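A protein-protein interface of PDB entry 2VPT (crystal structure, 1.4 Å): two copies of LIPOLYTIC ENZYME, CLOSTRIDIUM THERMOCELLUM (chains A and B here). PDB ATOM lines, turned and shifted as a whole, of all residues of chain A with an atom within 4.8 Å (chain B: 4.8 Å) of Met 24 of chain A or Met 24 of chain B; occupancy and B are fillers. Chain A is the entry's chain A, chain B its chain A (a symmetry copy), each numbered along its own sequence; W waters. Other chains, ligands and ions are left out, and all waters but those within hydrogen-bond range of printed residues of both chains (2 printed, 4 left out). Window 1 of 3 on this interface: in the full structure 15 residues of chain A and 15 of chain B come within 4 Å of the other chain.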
ATOM      1  N   GLU A  17     -33.693   7.912 -28.099  1.00  0.00           N
ATOM      2  CA  GLU A  17     -32.587   8.317 -27.239  1.00  0.00           C
ATOM      3  C   GLU A  17     -31.286   8.356 -28.032  1.00  0.00           C
ATOM      4  O   GLU A  17     -30.452   9.241 -27.809  1.00  0.00           O
ATOM      5  CB  GLU A  17     -32.478   7.422 -26.005  1.00  0.00           C
ATOM      6  CG  GLU A  17     -31.466   7.938 -24.974  1.00  0.00           C
ATOM      7  CD  GLU A  17     -31.653   7.347 -23.589  1.00  0.00           C
ATOM      8  OE1 GLU A  17     -32.131   6.196 -23.468  1.00  0.00           O
ATOM      9  OE2 GLU A  17     -31.303   8.057 -22.629  1.00  0.00           O
ATOM     10  N   GLY A  18     -31.132   7.417 -28.964  1.00  0.00           N
ATOM     11  CA  GLY A  18     -30.033   7.449 -29.927  1.00  0.00           C
ATOM     12  C   GLY A  18     -28.895   6.478 -29.720  1.00  0.00           C
ATOM     13  O   GLY A  18     -27.736   6.789 -29.996  1.00  0.00           O
ATOM     14  N   MET A  19     -29.190   5.271 -29.251  1.00  0.00           N
ATOM     15  CA  MET A  19     -28.157   4.259 -29.206  1.00  0.00           C
ATOM     16  C   MET A  19     -27.664   3.990 -30.629  1.00  0.00           C
ATOM     17  O   MET A  19     -28.352   4.272 -31.617  1.00  0.00           O
ATOM     18  CB  MET A  19     -28.663   2.974 -28.552  1.00  0.00           C
ATOM     19  CG  MET A  19     -28.923   3.121 -27.090  1.00  0.00           C
ATOM     20  SD  MET A  19     -29.233   1.422 -26.200  1.00  0.00           S
ATOM     21  CE  MET A  19     -28.844   1.916 -24.403  1.00  0.00           C
ATOM     22  N   GLY A  22     -23.773   8.340 -33.584  1.00  0.00           N
ATOM     23  CA  GLY A  22     -24.250   9.703 -33.481  1.00  0.00           C
ATOM     24  C   GLY A  22     -24.274  10.351 -32.107  1.00  0.00           C
ATOM     25  O   GLY A  22     -24.927  11.358 -31.932  1.00  0.00           O
ATOM     26  N   GLU A  23     -23.586   9.764 -31.133  1.00  0.00           N
ATOM     27  CA  GLU A  23     -23.422  10.381 -29.805  1.00  0.00           C
ATOM     28  C   GLU A  23     -24.745  10.707 -29.137  1.00  0.00           C
ATOM     29  O   GLU A  23     -24.918  11.765 -28.538  1.00  0.00           O
ATOM     30  CB  GLU A  23     -22.535  11.632 -29.889  1.00  0.00           C
ATOM     31  CG  GLU A  23     -21.186  11.326 -30.480  1.00  0.00           C
ATOM     32  CD  GLU A  23     -20.153  12.417 -30.332  1.00  0.00           C
ATOM     33  OE1 GLU A  23     -20.474  13.565 -29.922  1.00  0.00           O
ATOM     34  OE2 GLU A  23     -18.977  12.083 -30.640  1.00  0.00           O
ATOM     35  N   MET A  24     -25.672   9.763 -29.229  1.00  0.00           N
ATOM     36  CA  MET A  24     -26.964   9.864 -28.547  1.00  0.00           C
ATOM     37  C   MET A  24     -27.790  11.053 -29.014  1.00  0.00           C
ATOM     38  O   MET A  24     -28.561  11.647 -28.261  1.00  0.00           O
ATOM     39  CB  MET A  24     -26.791   9.846 -27.024  1.00  0.00           C
ATOM     40  CG  MET A  24     -25.884   8.751 -26.485  1.00  0.00           C
ATOM     41  SD  MET A  24     -26.526   6.927 -26.698  1.00  0.00           S
ATOM     42  CE  MET A  24     -28.044   7.329 -26.120  1.00  0.00           C
ATOM     43  N   GLY A  25     -27.639  11.375 -30.298  1.00  0.00           N
ATOM     44  CA  GLY A  25     -28.459  12.390 -30.946  1.00  0.00           C
ATOM     45  C   GLY A  25     -29.590  11.831 -31.795  1.00  0.00           C
ATOM     46  O   GLY A  25     -30.494  12.593 -32.170  1.00  0.00           O
ATOM     47  N   SER A  26     -29.577  10.526 -32.089  1.00  0.00           N
ATOM     48  CA  SER A  26     -30.654   9.924 -32.841  1.00  0.00           C
ATOM     49  C   SER A  26     -30.883  10.686 -34.147  1.00  0.00           C
ATOM     50  O   SER A  26     -29.923  11.180 -34.762  1.00  0.00           O
ATOM     51  CB  SER A  26     -31.902   9.872 -31.922  1.00  0.00           C
ATOM     52  OG  SER A  26     -33.071   9.395 -32.558  1.00  0.00           O
ATOM     53  N   ARG A  28     -32.522  13.349 -34.135  1.00  0.00           N
ATOM     54  CA  ARG A  28     -32.760  14.724 -33.683  1.00  0.00           C
ATOM     55  C   ARG A  28     -31.697  15.688 -34.209  1.00  0.00           C
ATOM     56  O   ARG A  28     -32.012  16.824 -34.560  1.00  0.00           O
ATOM     57  CB  ARG A  28     -32.871  14.773 -32.155  1.00  0.00           C
ATOM     58  CG  ARG A  28     -34.138  14.057 -31.653  1.00  0.00           C
ATOM     59  CD  ARG A  28     -34.161  13.832 -30.166  1.00  0.00           C
ATOM     60  NE  ARG A  28     -33.249  12.788 -29.710  1.00  0.00           N
ATOM     61  CZ  ARG A  28     -32.087  12.976 -29.081  1.00  0.00           C
ATOM     62  NH1 ARG A  28     -31.577  14.181 -28.843  1.00  0.00           N
ATOM     63  NH2 ARG A  28     -31.394  11.918 -28.724  1.00  0.00           N
ATOM     64  N   SER A  50     -29.454  14.558 -24.315  1.00  0.00           N
ATOM     65  CA  SER A  50     -28.323  13.861 -24.894  1.00  0.00           C
ATOM     66  C   SER A  50     -28.142  14.260 -26.341  1.00  0.00           C
ATOM     67  O   SER A  50     -29.103  14.628 -27.016  1.00  0.00           O
ATOM     68  CB  SER A  50     -28.494  12.345 -24.810  1.00  0.00           C
ATOM     69  OG  SER A  50     -29.548  11.850 -25.619  1.00  0.00           O
ATOM     70  N   GLY A  51     -26.914  14.141 -26.824  1.00  0.00           N
ATOM     71  CA  GLY A  51     -26.627  14.446 -28.196  1.00  0.00           C
ATOM     72  C   GLY A  51     -25.195  14.880 -28.379  1.00  0.00           C
ATOM     73  O   GLY A  51     -24.498  15.155 -27.407  1.00  0.00           O
ATOM     74  N   PRO A  52     -24.763  15.007 -29.636  1.00  0.00           N
ATOM     75  CA  PRO A  52     -23.436  15.535 -29.921  1.00  0.00           C
ATOM     76  C   PRO A  52     -23.397  17.025 -29.648  1.00  0.00           C
ATOM     77  O   PRO A  52     -24.429  17.674 -29.572  1.00  0.00           O
ATOM     78  CB  PRO A  52     -23.289  15.282 -31.411  1.00  0.00           C
ATOM     79  CG  PRO A  52     -24.678  15.341 -31.946  1.00  0.00           C
ATOM     80  CD  PRO A  52     -25.530  14.720 -30.867  1.00  0.00           C
ATOM     81  N   SER A  64     -34.207   4.369 -23.777  1.00  0.00           N
ATOM     82  CA  SER A  64     -33.691   3.084 -24.192  1.00  0.00           C
ATOM     83  C   SER A  64     -34.271   1.983 -23.316  1.00  0.00           C
ATOM     84  O   SER A  64     -34.303   2.105 -22.099  1.00  0.00           O
ATOM     85  CB  SER A  64     -32.168   3.064 -24.105  1.00  0.00           C
ATOM     86  OG  SER A  64     -31.618   4.036 -24.974  1.00  0.00           O
ATOM     87  N   GLU B  17     -21.821   7.953 -19.564  1.00  0.00           N
ATOM     88  CA  GLU B  17     -23.156   8.169 -20.108  1.00  0.00           C
ATOM     89  C   GLU B  17     -24.009   6.918 -19.933  1.00  0.00           C
ATOM     90  O   GLU B  17     -25.209   7.021 -19.652  1.00  0.00           O
ATOM     91  CB  GLU B  17     -23.104   8.627 -21.565  1.00  0.00           C
ATOM     92  CG  GLU B  17     -24.469   9.065 -22.109  1.00  0.00           C
ATOM     93  CD  GLU B  17     -24.379   9.921 -23.359  1.00  0.00           C
ATOM     94  OE1 GLU B  17     -23.418   9.765 -24.146  1.00  0.00           O
ATOM     95  OE2 GLU B  17     -25.296  10.743 -23.538  1.00  0.00           O
ATOM     96  N   GLY B  18     -23.384   5.751 -20.074  1.00  0.00           N
ATOM     97  CA  GLY B  18     -24.025   4.480 -19.743  1.00  0.00           C
ATOM     98  C   GLY B  18     -24.481   3.609 -20.891  1.00  0.00           C
ATOM     99  O   GLY B  18     -25.503   2.927 -20.802  1.00  0.00           O
ATOM    100  N   MET B  19     -23.730   3.586 -21.986  1.00  0.00           N
ATOM    101  CA  MET B  19     -24.037   2.634 -23.032  1.00  0.00           C
ATOM    102  C   MET B  19     -23.907   1.218 -22.468  1.00  0.00           C
ATOM    103  O   MET B  19     -23.236   0.984 -21.456  1.00  0.00           O
ATOM    104  CB  MET B  19     -23.127   2.826 -24.244  1.00  0.00           C
ATOM    105  CG  MET B  19     -23.390   4.095 -24.984  1.00  0.00           C
ATOM    106  SD  MET B  19     -22.482   4.175 -26.699  1.00  0.00           S
ATOM    107  CE  MET B  19     -23.541   5.494 -27.571  1.00  0.00           C
ATOM    108  N   GLY B  22     -28.541  -1.122 -18.489  1.00  0.00           N
ATOM    109  CA  GLY B  22     -28.908  -0.205 -17.429  1.00  0.00           C
ATOM    110  C   GLY B  22     -29.603   1.090 -17.812  1.00  0.00           C
ATOM    111  O   GLY B  22     -29.658   1.998 -17.011  1.00  0.00           O
ATOM    112  N   GLU B  23     -30.108   1.184 -19.038  1.00  0.00           N
ATOM    113  CA  GLU B  23     -30.925   2.332 -19.466  1.00  0.00           C
ATOM    114  C   GLU B  23     -30.215   3.662 -19.289  1.00  0.00           C
ATOM    115  O   GLU B  23     -30.798   4.648 -18.846  1.00  0.00           O
ATOM    116  CB  GLU B  23     -32.278   2.341 -18.739  1.00  0.00           C
ATOM    117  CG  GLU B  23     -33.042   1.062 -18.956  1.00  0.00           C
ATOM    118  CD  GLU B  23     -34.490   1.094 -18.531  1.00  0.00           C
ATOM    119  OE1 GLU B  23     -34.951   2.059 -17.864  1.00  0.00           O
ATOM    120  OE2 GLU B  23     -35.175   0.103 -18.899  1.00  0.00           O
ATOM    121  N   MET B  24     -28.944   3.678 -19.671  1.00  0.00           N
ATOM    122  CA  MET B  24     -28.144   4.904 -19.676  1.00  0.00           C
ATOM    123  C   MET B  24     -27.984   5.515 -18.291  1.00  0.00           C
ATOM    124  O   MET B  24     -27.882   6.728 -18.122  1.00  0.00           O
ATOM    125  CB  MET B  24     -28.685   5.917 -20.692  1.00  0.00           C
ATOM    126  CG  MET B  24     -28.980   5.357 -22.074  1.00  0.00           C
ATOM    127  SD  MET B  24     -27.440   4.754 -23.099  1.00  0.00           S
ATOM    128  CE  MET B  24     -26.588   6.153 -22.758  1.00  0.00           C
ATOM    129  N   GLY B  25     -27.928   4.636 -17.291  1.00  0.00           N
ATOM    130  CA  GLY B  25     -27.632   5.035 -15.922  1.00  0.00           C
ATOM    131  C   GLY B  25     -26.198   4.773 -15.491  1.00  0.00           C
ATOM    132  O   GLY B  25     -25.773   5.307 -14.456  1.00  0.00           O
ATOM    133  N   SER B  26     -25.437   3.988 -16.263  1.00  0.00           N
ATOM    134  CA  SER B  26     -24.049   3.749 -15.940  1.00  0.00           C
ATOM    135  C   SER B  26     -23.916   3.247 -14.502  1.00  0.00           C
ATOM    136  O   SER B  26     -24.783   2.502 -14.015  1.00  0.00           O
ATOM    137  CB  SER B  26     -23.266   5.059 -16.217  1.00  0.00           C
ATOM    138  OG  SER B  26     -21.901   5.008 -15.851  1.00  0.00           O
ATOM    139  N   ARG B  28     -24.012   5.273 -12.123  1.00  0.00           N
ATOM    140  CA  ARG B  28     -24.671   6.323 -11.339  1.00  0.00           C
ATOM    141  C   ARG B  28     -25.894   5.793 -10.591  1.00  0.00           C
ATOM    142  O   ARG B  28     -26.148   6.193  -9.457  1.00  0.00           O
ATOM    143  CB  ARG B  28     -25.020   7.519 -12.232  1.00  0.00           C
ATOM    144  CG  ARG B  28     -23.757   8.247 -12.727  1.00  0.00           C
ATOM    145  CD  ARG B  28     -24.022   9.248 -13.818  1.00  0.00           C
ATOM    146  NE  ARG B  28     -24.325   8.647 -15.113  1.00  0.00           N
ATOM    147  CZ  ARG B  28     -25.529   8.571 -15.685  1.00  0.00           C
ATOM    148  NH1 ARG B  28     -26.641   8.996 -15.092  1.00  0.00           N
ATOM    149  NH2 ARG B  28     -25.622   8.009 -16.868  1.00  0.00           N
ATOM    150  N   SER B  50     -29.772  11.339 -18.233  1.00  0.00           N
ATOM    151  CA  SER B  50     -30.155  10.017 -18.683  1.00  0.00           C
ATOM    152  C   SER B  50     -30.122   9.036 -17.533  1.00  0.00           C
ATOM    153  O   SER B  50     -29.362   9.212 -16.581  1.00  0.00           O
ATOM    154  CB  SER B  50     -29.237   9.514 -19.797  1.00  0.00           C
ATOM    155  OG  SER B  50     -27.909   9.268 -19.366  1.00  0.00           O
ATOM    156  N   GLY B  51     -30.915   7.982 -17.649  1.00  0.00           N
ATOM    157  CA  GLY B  51     -30.937   6.959 -16.643  1.00  0.00           C
ATOM    158  C   GLY B  51     -32.269   6.255 -16.597  1.00  0.00           C
ATOM    159  O   GLY B  51     -33.238   6.715 -17.194  1.00  0.00           O
ATOM    160  N   PRO B  52     -32.343   5.164 -15.832  1.00  0.00           N
ATOM    161  CA  PRO B  52     -33.614   4.481 -15.626  1.00  0.00           C
ATOM    162  C   PRO B  52     -34.508   5.302 -14.720  1.00  0.00           C
ATOM    163  O   PRO B  52     -34.043   6.185 -14.015  1.00  0.00           O
ATOM    164  CB  PRO B  52     -33.195   3.205 -14.915  1.00  0.00           C
ATOM    165  CG  PRO B  52     -31.965   3.576 -14.161  1.00  0.00           C
ATOM    166  CD  PRO B  52     -31.243   4.548 -15.062  1.00  0.00           C
ATOM    167  N   SER B  64     -20.698   9.851 -24.726  1.00  0.00           N
ATOM    168  CA  SER B  64     -20.320   8.720 -25.543  1.00  0.00           C
ATOM    169  C   SER B  64     -19.507   9.191 -26.740  1.00  0.00           C
ATOM    170  O   SER B  64     -19.875  10.149 -27.406  1.00  0.00           O
ATOM    171  CB  SER B  64     -21.557   7.968 -26.023  1.00  0.00           C
ATOM    172  OG  SER B  64     -22.280   7.462 -24.917  1.00  0.00           O
HETATM  173  O   HOH W   1     -24.898  12.570 -25.465  1.00  0.00           O
HETATM  174  O   HOH W   2     -32.072   7.228 -20.193  1.00  0.00           O
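Of the 13 printed residues of chain B, 6 touch a printed residue of chain A. Hydrophobic or aromatic side chains of chain B that line the printed part of chain A: Met 19 and Met 24. Among the printed residues, 9 pairs touch across the chains.
Water W1 lies within hydrogen-bond range of the side-chain carboxylate of Glu 17 of chain B (2.7 Å), the backbone NH of Gly 51 of chain A (2.9 Å) and the backbone carbonyl oxygen of Glu 23 of chain A (3.2 Å). Water W2 lies within hydrogen-bond range of the side-chain carboxylate of Glu 17 of chain A (2.7 Å), the backbone NH of Gly 51 of chain B (2.9 Å) and the backbone carbonyl oxygen of Glu 23 of chain B (3.2 Å).
Glu 17 of chain A touches Met 24 of chain B, and with the chains exchanged Met 24 of chain A touches Glu 17 of chain B. Glu 17 of chain A touches Ser 50 of chain B, and with the chains exchanged Ser 50 of chain A touches Glu 17 of chain B. Met 19 of chain A touches Met 24 of chain B, and with the chains exchanged Met 24 of chain A touches Met 19 of chain B. Met 24 of chain B touches its own counterpart, Met 24 of chain A. Positions printed for both chains: 17, 18, 19, 22, 23, 24, 25, 26, 28, 50, 51, 52 and 64.
Of the printed residues of chain B, Glu 23 of chain A touches Ser 64 (3.5 Å). Met 24 of chain A touches three residues of chain B. Printed residues of chain B within 4 Å of Ser 50 of chain A: Glu 17. Of the printed residues of chain A, Glu 17 of chain B touches Met 24 (3.5 Å) and Ser 50 (3.8 Å). Met 24 of chain B touches just these residues of chain A: Glu 17, Met 19 and Met 24. The nearest printed residue of chain B that does not touch Ser 64 of chain A is Met 24 of chain B (4.1 Å).
Among the printed residues, pairs that only touch across the chains: Met 24 of chain A with Met 19 of chain B (3.4 Å), Met 19 of chain A with Met 24 of chain B (3.4 Å), Glu 23 of chain A with Ser 64 of chain B (3.5 Å), Ser 64 of chain A with Glu 23 of chain B (3.5 Å), Glu 17 of chain A with Met 24 of chain B (3.5 Å), Met 24 of chain A with Glu 17 of chain B (3.5 Å), Glu 17 of chain A with Ser 50 of chain B (3.8 Å), Ser 50 of chain A with Glu 17 of chain B (3.8 Å) and Met 24 of chain A with Met 24 of chain B (3.8 Å).
The backbone carbonyl oxygen (O) of Ser 50 of chain A is in hydrogen-bond range of the guanidinium group (NH1) of Arg 28 of chain A (3.1 Å). The backbone carbonyl oxygen (O) of Met 24 of chain A lies within hydrogen-bond range of the backbone NH (N) of Gly 51 of chain A (3.3 Å). OG of Ser 50 of chain A is in hydrogen-bond range of O of Met 24 of chain A. The backbone carbonyl oxygen of Glu 17 of chain B sits at hydrogen-bond distance from the guanidinium group of Arg 28 of chain B. The guanidinium group of Arg 28 of chain A sits at hydrogen-bond distance from the backbone carbonyl oxygen of Glu 17 of chain A (3.0 Å). The side-chain carboxylate (OE1) of Glu 17 of chain A lies within hydrogen-bond range of the side-chain hydroxyl (OG) of Ser 64 of chain A, 2.7 Å away.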
